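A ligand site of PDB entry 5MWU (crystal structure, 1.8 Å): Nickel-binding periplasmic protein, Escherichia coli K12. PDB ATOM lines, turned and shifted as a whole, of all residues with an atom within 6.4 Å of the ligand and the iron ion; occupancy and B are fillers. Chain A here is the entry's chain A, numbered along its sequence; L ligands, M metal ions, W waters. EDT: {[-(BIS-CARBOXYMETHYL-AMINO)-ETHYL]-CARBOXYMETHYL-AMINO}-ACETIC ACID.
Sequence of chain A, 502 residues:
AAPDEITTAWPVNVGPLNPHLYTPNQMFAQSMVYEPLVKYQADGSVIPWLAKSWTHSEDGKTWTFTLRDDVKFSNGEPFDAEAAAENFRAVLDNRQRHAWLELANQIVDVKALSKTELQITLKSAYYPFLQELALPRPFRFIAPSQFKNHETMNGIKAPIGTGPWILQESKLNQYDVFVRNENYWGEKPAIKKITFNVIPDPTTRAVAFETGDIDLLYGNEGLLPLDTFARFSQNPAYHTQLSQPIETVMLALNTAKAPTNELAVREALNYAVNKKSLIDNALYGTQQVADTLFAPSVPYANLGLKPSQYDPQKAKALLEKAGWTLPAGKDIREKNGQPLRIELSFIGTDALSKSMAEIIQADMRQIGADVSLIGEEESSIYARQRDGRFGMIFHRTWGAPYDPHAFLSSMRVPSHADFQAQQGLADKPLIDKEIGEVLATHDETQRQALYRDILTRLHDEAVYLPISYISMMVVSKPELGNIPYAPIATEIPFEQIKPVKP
Water W1 lies within hydrogen-bond range of OH of Tyr 402 (2.6 Å), O17 of the ligand (2.6 Å) and O of Arg 137 (2.7 Å). Water W4 bridges an oxygen (O14) of the ligand (2.8 Å) and the backbone NH (N) of Thr 23 (3.2 Å).
The side-chain sulfur (SD) of Met 27 sits close to an oxygen (O17) of the ligand (3.6 Å). Merely in contact with the ligand: Tyr 22, Trp 100, Trp 398, Thr 490 and Tyr 402. Within 4 Å of the ligand: Tyr 22, Met 27, Arg 97, Trp 100, Arg 137, Trp 398, Tyr 402 and Thr 490.
An oxygen (O20) of the ligand binds the iron ion. Water W5 is bound to the iron ion (2.1 Å). O13 of the ligand is bound to the iron ion. The iron ion is bound by O16 of the ligand (2.2 Å). O18 of the ligand binds the iron ion (2.2 Å). N3 of the ligand is bound to the iron ion. N8 of the ligand binds the iron ion (2.3 Å).
OG1 of Thr 490 is in hydrogen-bond range of SD of Met 27, 3.8 Å away. OH of Tyr 402 is in hydrogen-bond range of SD of Met 27. The side-chain hydroxyl of Tyr 22 is in hydrogen-bond range of the indole nitrogen of Trp 100, at 2.9 Å.
No residue comes within 4 Å of the iron ion.
The guanidinium group of Arg 97 is in salt-bridge range of an oxygen (O14) of the ligand (2.8 Å). The guanidinium group (NE) of Arg 137 lies within salt-bridge range of an oxygen (O17) of the ligand, 3.0 Å away.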
ATOM      1  N   TYR A  22      25.622  25.083   3.842  1.00  0.00           N
ATOM      2  CA  TYR A  22      26.650  25.166   2.790  1.00  0.00           C
ATOM      3  C   TYR A  22      27.211  26.559   2.807  1.00  0.00           C
ATOM      4  O   TYR A  22      27.473  27.078   3.882  1.00  0.00           O
ATOM      5  CB  TYR A  22      26.032  24.679   1.435  1.00  0.00           C
ATOM      6  CG  TYR A  22      25.548  23.301   1.478  1.00  0.00           C
ATOM      7  CD1 TYR A  22      24.258  23.032   1.943  1.00  0.00           C
ATOM      8  CD2 TYR A  22      26.347  22.282   1.162  1.00  0.00           C
ATOM      9  CE1 TYR A  22      23.800  21.781   2.050  1.00  0.00           C
ATOM     10  CE2 TYR A  22      25.941  20.980   1.293  1.00  0.00           C
ATOM     11  CZ  TYR A  22      24.610  20.733   1.706  1.00  0.00           C
ATOM     12  OH  TYR A  22      24.170  19.443   1.804  1.00  0.00           O
ATOM     13  N   THR A  23      27.398  27.233   1.646  1.00  0.00           N
ATOM     14  CA  THR A  23      27.878  28.576   1.631  1.00  0.00           C
ATOM     15  C   THR A  23      27.129  29.479   2.588  1.00  0.00           C
ATOM     16  O   THR A  23      25.896  29.357   2.709  1.00  0.00           O
ATOM     17  CB  THR A  23      27.859  29.169   0.152  1.00  0.00           C
ATOM     18  OG1 THR A  23      28.554  30.425   0.165  1.00  0.00           O
ATOM     19  CG2 THR A  23      26.506  29.407  -0.336  1.00  0.00           C
ATOM     20  N   MET A  27      34.011  24.111   3.841  1.00  0.00           N
ATOM     21  CA  MET A  27      34.094  22.701   4.226  1.00  0.00           C
ATOM     22  C   MET A  27      35.301  22.320   5.049  1.00  0.00           C
ATOM     23  O   MET A  27      35.214  21.550   6.089  1.00  0.00           O
ATOM     24  CB  MET A  27      34.033  21.745   3.008  1.00  0.00           C
ATOM     25  CG  MET A  27      32.612  21.458   2.523  1.00  0.00           C
ATOM     26  SD  MET A  27      32.573  20.372   1.061  1.00  0.00           S
ATOM     27  CE  MET A  27      33.428  21.428  -0.096  1.00  0.00           C
ATOM     28  N   ARG A  97      17.262  20.901   0.856  1.00  0.00           N
ATOM     29  CA  ARG A  97      18.589  21.480   0.604  1.00  0.00           C
ATOM     30  C   ARG A  97      19.663  20.468   0.317  1.00  0.00           C
ATOM     31  O   ARG A  97      20.684  20.811  -0.341  1.00  0.00           O
ATOM     32  CB  ARG A  97      18.967  22.438   1.726  1.00  0.00           C
ATOM     33  CG  ARG A  97      20.270  23.137   1.509  1.00  0.00           C
ATOM     34  CD  ARG A  97      20.216  24.144   0.359  1.00  0.00           C
ATOM     35  NE  ARG A  97      21.541  24.735   0.035  1.00  0.00           N
ATOM     36  CZ  ARG A  97      22.454  24.179  -0.757  1.00  0.00           C
ATOM     37  NH1 ARG A  97      22.316  22.947  -1.215  1.00  0.00           N
ATOM     38  NH2 ARG A  97      23.591  24.830  -1.039  1.00  0.00           N
ATOM     39  N   TRP A 100      21.075  16.944  -3.594  1.00  0.00           N
ATOM     40  CA  TRP A 100      22.196  16.538  -4.375  1.00  0.00           C
ATOM     41  C   TRP A 100      22.810  15.292  -3.810  1.00  0.00           C
ATOM     42  O   TRP A 100      23.409  14.535  -4.542  1.00  0.00           O
ATOM     43  CB  TRP A 100      23.202  17.699  -4.423  1.00  0.00           C
ATOM     44  CG  TRP A 100      23.825  17.967  -3.077  1.00  0.00           C
ATOM     45  CD1 TRP A 100      23.399  18.828  -2.120  1.00  0.00           C
ATOM     46  CD2 TRP A 100      24.963  17.312  -2.544  1.00  0.00           C
ATOM     47  NE1 TRP A 100      24.211  18.718  -1.013  1.00  0.00           N
ATOM     48  CE2 TRP A 100      25.195  17.839  -1.259  1.00  0.00           C
ATOM     49  CE3 TRP A 100      25.843  16.389  -3.053  1.00  0.00           C
ATOM     50  CZ2 TRP A 100      26.230  17.406  -0.448  1.00  0.00           C
ATOM     51  CZ3 TRP A 100      26.876  15.975  -2.269  1.00  0.00           C
ATOM     52  CH2 TRP A 100      27.050  16.469  -0.955  1.00  0.00           C
ATOM     53  N   LEU A 135      31.474  12.419   4.874  1.00  0.00           N
ATOM     54  CA  LEU A 135      31.681  13.672   4.213  1.00  0.00           C
ATOM     55  C   LEU A 135      31.800  14.851   5.243  1.00  0.00           C
ATOM     56  O   LEU A 135      31.244  14.731   6.331  1.00  0.00           O
ATOM     57  CB  LEU A 135      30.551  13.991   3.256  1.00  0.00           C
ATOM     58  CG  LEU A 135      30.424  13.017   2.055  1.00  0.00           C
ATOM     59  CD1 LEU A 135      29.242  13.413   1.181  1.00  0.00           C
ATOM     60  CD2 LEU A 135      31.708  12.969   1.290  1.00  0.00           C
ATOM     61  N   PRO A 136      32.462  15.984   4.860  1.00  0.00           N
ATOM     62  CA  PRO A 136      32.609  17.150   5.710  1.00  0.00           C
ATOM     63  C   PRO A 136      31.201  17.575   6.218  1.00  0.00           C
ATOM     64  O   PRO A 136      31.099  18.105   7.345  1.00  0.00           O
ATOM     65  CB  PRO A 136      33.164  18.199   4.742  1.00  0.00           C
ATOM     66  CG  PRO A 136      34.063  17.376   3.903  1.00  0.00           C
ATOM     67  CD  PRO A 136      33.246  16.157   3.604  1.00  0.00           C
ATOM     68  N   ARG A 137      30.194  17.521   5.325  1.00  0.00           N
ATOM     69  CA  ARG A 137      28.804  17.955   5.597  1.00  0.00           C
ATOM     70  C   ARG A 137      27.882  17.122   4.731  1.00  0.00           C
ATOM     71  O   ARG A 137      28.262  16.753   3.639  1.00  0.00           O
ATOM     72  CB  ARG A 137      28.624  19.448   5.370  1.00  0.00           C
ATOM     73  CG  ARG A 137      28.938  19.916   3.954  1.00  0.00           C
ATOM     74  CD  ARG A 137      29.199  21.398   3.910  1.00  0.00           C
ATOM     75  NE  ARG A 137      29.356  21.883   2.529  1.00  0.00           N
ATOM     76  CZ  ARG A 137      29.721  23.111   2.218  1.00  0.00           C
ATOM     77  NH1 ARG A 137      30.084  23.985   3.126  1.00  0.00           N
ATOM     78  NH2 ARG A 137      29.739  23.490   0.965  1.00  0.00           N
ATOM     79  N   PRO A 138      26.642  16.926   5.137  1.00  0.00           N
ATOM     80  CA  PRO A 138      26.054  17.560   6.329  1.00  0.00           C
ATOM     81  C   PRO A 138      25.983  16.658   7.558  1.00  0.00           C
ATOM     82  O   PRO A 138      25.581  17.146   8.572  1.00  0.00           O
ATOM     83  CB  PRO A 138      24.626  17.809   5.887  1.00  0.00           C
ATOM     84  CG  PRO A 138      24.347  16.625   5.009  1.00  0.00           C
ATOM     85  CD  PRO A 138      25.623  16.376   4.248  1.00  0.00           C
ATOM     86  N   GLU A 247      40.918  15.935  -8.864  1.00  0.00           N
ATOM     87  CA  GLU A 247      39.620  16.062  -9.537  1.00  0.00           C
ATOM     88  C   GLU A 247      39.836  16.642 -10.918  1.00  0.00           C
ATOM     89  O   GLU A 247      40.947  17.117 -11.240  1.00  0.00           O
ATOM     90  CB  GLU A 247      38.682  16.949  -8.694  1.00  0.00           C
ATOM     91  CG  GLU A 247      39.123  18.401  -8.626  1.00  0.00           C
ATOM     92  CD  GLU A 247      38.683  19.135  -7.344  1.00  0.00           C
ATOM     93  OE1 GLU A 247      38.365  18.516  -6.292  1.00  0.00           O
ATOM     94  OE2 GLU A 247      38.610  20.379  -7.400  1.00  0.00           O
ATOM     95  N   GLN A 385      24.516  28.175 -14.269  1.00  0.00           N
ATOM     96  CA  GLN A 385      24.666  26.723 -14.147  1.00  0.00           C
ATOM     97  C   GLN A 385      23.343  26.076 -13.756  1.00  0.00           C
ATOM     98  O   GLN A 385      22.994  25.004 -14.273  1.00  0.00           O
ATOM     99  CB  GLN A 385      25.709  26.401 -13.082  1.00  0.00           C
ATOM    100  CG  GLN A 385      27.115  26.669 -13.516  1.00  0.00           C
ATOM    101  CD  GLN A 385      28.178  26.197 -12.488  1.00  0.00           C
ATOM    102  OE1 GLN A 385      27.876  26.018 -11.321  1.00  0.00           O
ATOM    103  NE2 GLN A 385      29.378  25.938 -12.959  1.00  0.00           N
ATOM    104  N   HIS A 395      33.593  24.000 -15.210  1.00  0.00           N
ATOM    105  CA  HIS A 395      32.966  23.171 -14.203  1.00  0.00           C
ATOM    106  C   HIS A 395      34.086  22.294 -13.688  1.00  0.00           C
ATOM    107  O   HIS A 395      35.234  22.226 -14.265  1.00  0.00           O
ATOM    108  CB  HIS A 395      31.814  22.409 -14.858  1.00  0.00           C
ATOM    109  CG  HIS A 395      30.869  21.719 -13.888  1.00  0.00           C
ATOM    110  ND1 HIS A 395      30.721  22.101 -12.568  1.00  0.00           N
ATOM    111  CD2 HIS A 395      30.134  20.588 -14.033  1.00  0.00           C
ATOM    112  CE1 HIS A 395      29.868  21.290 -11.967  1.00  0.00           C
ATOM    113  NE2 HIS A 395      29.473  20.373 -12.840  1.00  0.00           N
ATOM    114  N   ARG A 396      33.791  21.555 -12.634  1.00  0.00           N
ATOM    115  CA  ARG A 396      34.742  20.662 -12.046  1.00  0.00           C
ATOM    116  C   ARG A 396      34.065  19.527 -11.331  1.00  0.00           C
ATOM    117  O   ARG A 396      32.916  19.613 -10.857  1.00  0.00           O
ATOM    118  CB  ARG A 396      35.742  21.393 -11.117  1.00  0.00           C
ATOM    119  CG  ARG A 396      35.144  22.094  -9.938  1.00  0.00           C
ATOM    120  CD  ARG A 396      36.080  23.160  -9.327  1.00  0.00           C
ATOM    121  NE  ARG A 396      37.406  22.641  -8.949  1.00  0.00           N
ATOM    122  CZ  ARG A 396      38.559  23.217  -9.288  1.00  0.00           C
ATOM    123  NH1 ARG A 396      38.624  24.364  -9.947  1.00  0.00           N
ATOM    124  NH2 ARG A 396      39.684  22.676  -8.881  1.00  0.00           N
ATOM    125  N   THR A 397      34.767  18.408 -11.248  1.00  0.00           N
ATOM    126  CA  THR A 397      34.318  17.317 -10.405  1.00  0.00           C
ATOM    127  C   THR A 397      34.730  17.568  -8.945  1.00  0.00           C
ATOM    128  O   THR A 397      35.248  18.636  -8.599  1.00  0.00           O
ATOM    129  CB  THR A 397      34.737  15.903 -10.860  1.00  0.00           C
ATOM    130  OG1 THR A 397      36.141  15.686 -10.669  1.00  0.00           O
ATOM    131  CG2 THR A 397      34.312  15.657 -12.324  1.00  0.00           C
ATOM    132  N   TRP A 398      34.399  16.630  -8.063  1.00  0.00           N
ATOM    133  CA  TRP A 398      34.416  16.970  -6.620  1.00  0.00           C
ATOM    134  C   TRP A 398      35.509  16.304  -5.837  1.00  0.00           C
ATOM    135  O   TRP A 398      35.642  16.553  -4.684  1.00  0.00           O
ATOM    136  CB  TRP A 398      33.024  16.643  -6.040  1.00  0.00           C
ATOM    137  CG  TRP A 398      31.908  17.512  -6.587  1.00  0.00           C
ATOM    138  CD1 TRP A 398      32.039  18.684  -7.219  1.00  0.00           C
ATOM    139  CD2 TRP A 398      30.471  17.289  -6.451  1.00  0.00           C
ATOM    140  NE1 TRP A 398      30.798  19.202  -7.526  1.00  0.00           N
ATOM    141  CE2 TRP A 398      29.827  18.354  -7.078  1.00  0.00           C
ATOM    142  CE3 TRP A 398      29.710  16.257  -5.937  1.00  0.00           C
ATOM    143  CZ2 TRP A 398      28.444  18.447  -7.163  1.00  0.00           C
ATOM    144  CZ3 TRP A 398      28.278  16.356  -6.036  1.00  0.00           C
ATOM    145  CH2 TRP A 398      27.692  17.424  -6.644  1.00  0.00           C
ATOM    146  N   TYR A 402      33.537  11.824  -3.288  1.00  0.00           N
ATOM    147  CA  TYR A 402      32.437  12.133  -4.189  1.00  0.00           C
ATOM    148  C   TYR A 402      32.493  11.500  -5.588  1.00  0.00           C
ATOM    149  O   TYR A 402      31.416  11.174  -6.190  1.00  0.00           O
ATOM    150  CB  TYR A 402      32.292  13.668  -4.400  1.00  0.00           C
ATOM    151  CG  TYR A 402      32.237  14.459  -3.148  1.00  0.00           C
ATOM    152  CD1 TYR A 402      31.001  14.728  -2.531  1.00  0.00           C
ATOM    153  CD2 TYR A 402      33.411  14.990  -2.532  1.00  0.00           C
ATOM    154  CE1 TYR A 402      30.961  15.487  -1.332  1.00  0.00           C
ATOM    155  CE2 TYR A 402      33.339  15.737  -1.346  1.00  0.00           C
ATOM    156  CZ  TYR A 402      32.124  15.997  -0.774  1.00  0.00           C
ATOM    157  OH  TYR A 402      32.065  16.733   0.406  1.00  0.00           O
ATOM    158  N   HIS A 416      21.451  21.801 -11.181  1.00  0.00           N
ATOM    159  CA  HIS A 416      22.895  21.720 -11.210  1.00  0.00           C
ATOM    160  C   HIS A 416      23.347  21.733 -12.664  1.00  0.00           C
ATOM    161  O   HIS A 416      22.626  21.322 -13.578  1.00  0.00           O
ATOM    162  CB  HIS A 416      23.365  20.444 -10.536  1.00  0.00           C
ATOM    163  CG  HIS A 416      23.252  20.450  -9.043  1.00  0.00           C
ATOM    164  ND1 HIS A 416      24.068  19.674  -8.245  1.00  0.00           N
ATOM    165  CD2 HIS A 416      22.462  21.158  -8.198  1.00  0.00           C
ATOM    166  CE1 HIS A 416      23.779  19.899  -6.973  1.00  0.00           C
ATOM    167  NE2 HIS A 416      22.810  20.800  -6.922  1.00  0.00           N
ATOM    168  N   THR A 490      38.404  18.037  -0.153  1.00  0.00           N
ATOM    169  CA  THR A 490      38.053  19.351   0.412  1.00  0.00           C
ATOM    170  C   THR A 490      38.530  19.609   1.839  1.00  0.00           C
ATOM    171  O   THR A 490      38.306  20.665   2.405  1.00  0.00           O
ATOM    172  CB  THR A 490      36.528  19.549   0.382  1.00  0.00           C
ATOM    173  OG1 THR A 490      35.859  18.484   1.042  1.00  0.00           O
ATOM    174  CG2 THR A 490      36.003  19.520  -1.065  1.00  0.00           C
HETATM  175  O20 EDT L   1      31.558  21.709  -2.859  1.00  0.00           O
HETATM  176  C5  EDT L   1      32.107  20.606  -3.232  1.00  0.00           C
HETATM  177  O19 EDT L   1      33.319  20.382  -3.465  1.00  0.00           O
HETATM  178  C4  EDT L   1      31.253  19.439  -3.455  1.00  0.00           C
HETATM  179  N3  EDT L   1      29.918  19.708  -2.883  1.00  0.00           N
HETATM  180  C2  EDT L   1      29.884  19.195  -1.513  1.00  0.00           C
HETATM  181  C1  EDT L   1      29.276  20.205  -0.559  1.00  0.00           C
HETATM  182  O18 EDT L   1      29.097  21.437  -0.851  1.00  0.00           O
HETATM  183  O17 EDT L   1      29.030  19.689   0.549  1.00  0.00           O
HETATM  184  C6  EDT L   1      28.863  19.031  -3.684  1.00  0.00           C
HETATM  185  C7  EDT L   1      27.465  19.518  -3.389  1.00  0.00           C
HETATM  186  N8  EDT L   1      27.554  20.977  -3.532  1.00  0.00           N
HETATM  187  C9  EDT L   1      27.232  21.441  -4.879  1.00  0.00           C
HETATM  188  C10 EDT L   1      28.504  21.836  -5.668  1.00  0.00           C
HETATM  189  O16 EDT L   1      29.565  22.063  -5.064  1.00  0.00           O
HETATM  190  O15 EDT L   1      28.481  21.903  -6.918  1.00  0.00           O
HETATM  191  C11 EDT L   1      26.623  21.640  -2.581  1.00  0.00           C
HETATM  192  C12 EDT L   1      26.903  23.110  -2.492  1.00  0.00           C
HETATM  193  O13 EDT L   1      28.102  23.498  -2.701  1.00  0.00           O
HETATM  194  O14 EDT L   1      25.954  23.853  -2.181  1.00  0.00           O
HETATM  195 FE    FE M   1      29.558  21.976  -2.899  1.00  0.00          FE
HETATM  196  O   HOH W   1      29.810  17.352   1.463  1.00  0.00           O
HETATM  197  O   HOH W   2      27.294  20.921  -9.346  1.00  0.00           O
HETATM  198  O   HOH W   3      29.479  26.560  -2.441  1.00  0.00           O
HETATM  199  O   HOH W   4      26.898  26.334  -1.358  1.00  0.00           O
HETATM  200  O   HOH W   5      30.251  23.864  -2.299  1.00  0.00           O
HETATM  201  O   HOH W   6      34.833  22.653  -3.047  1.00  0.00           O
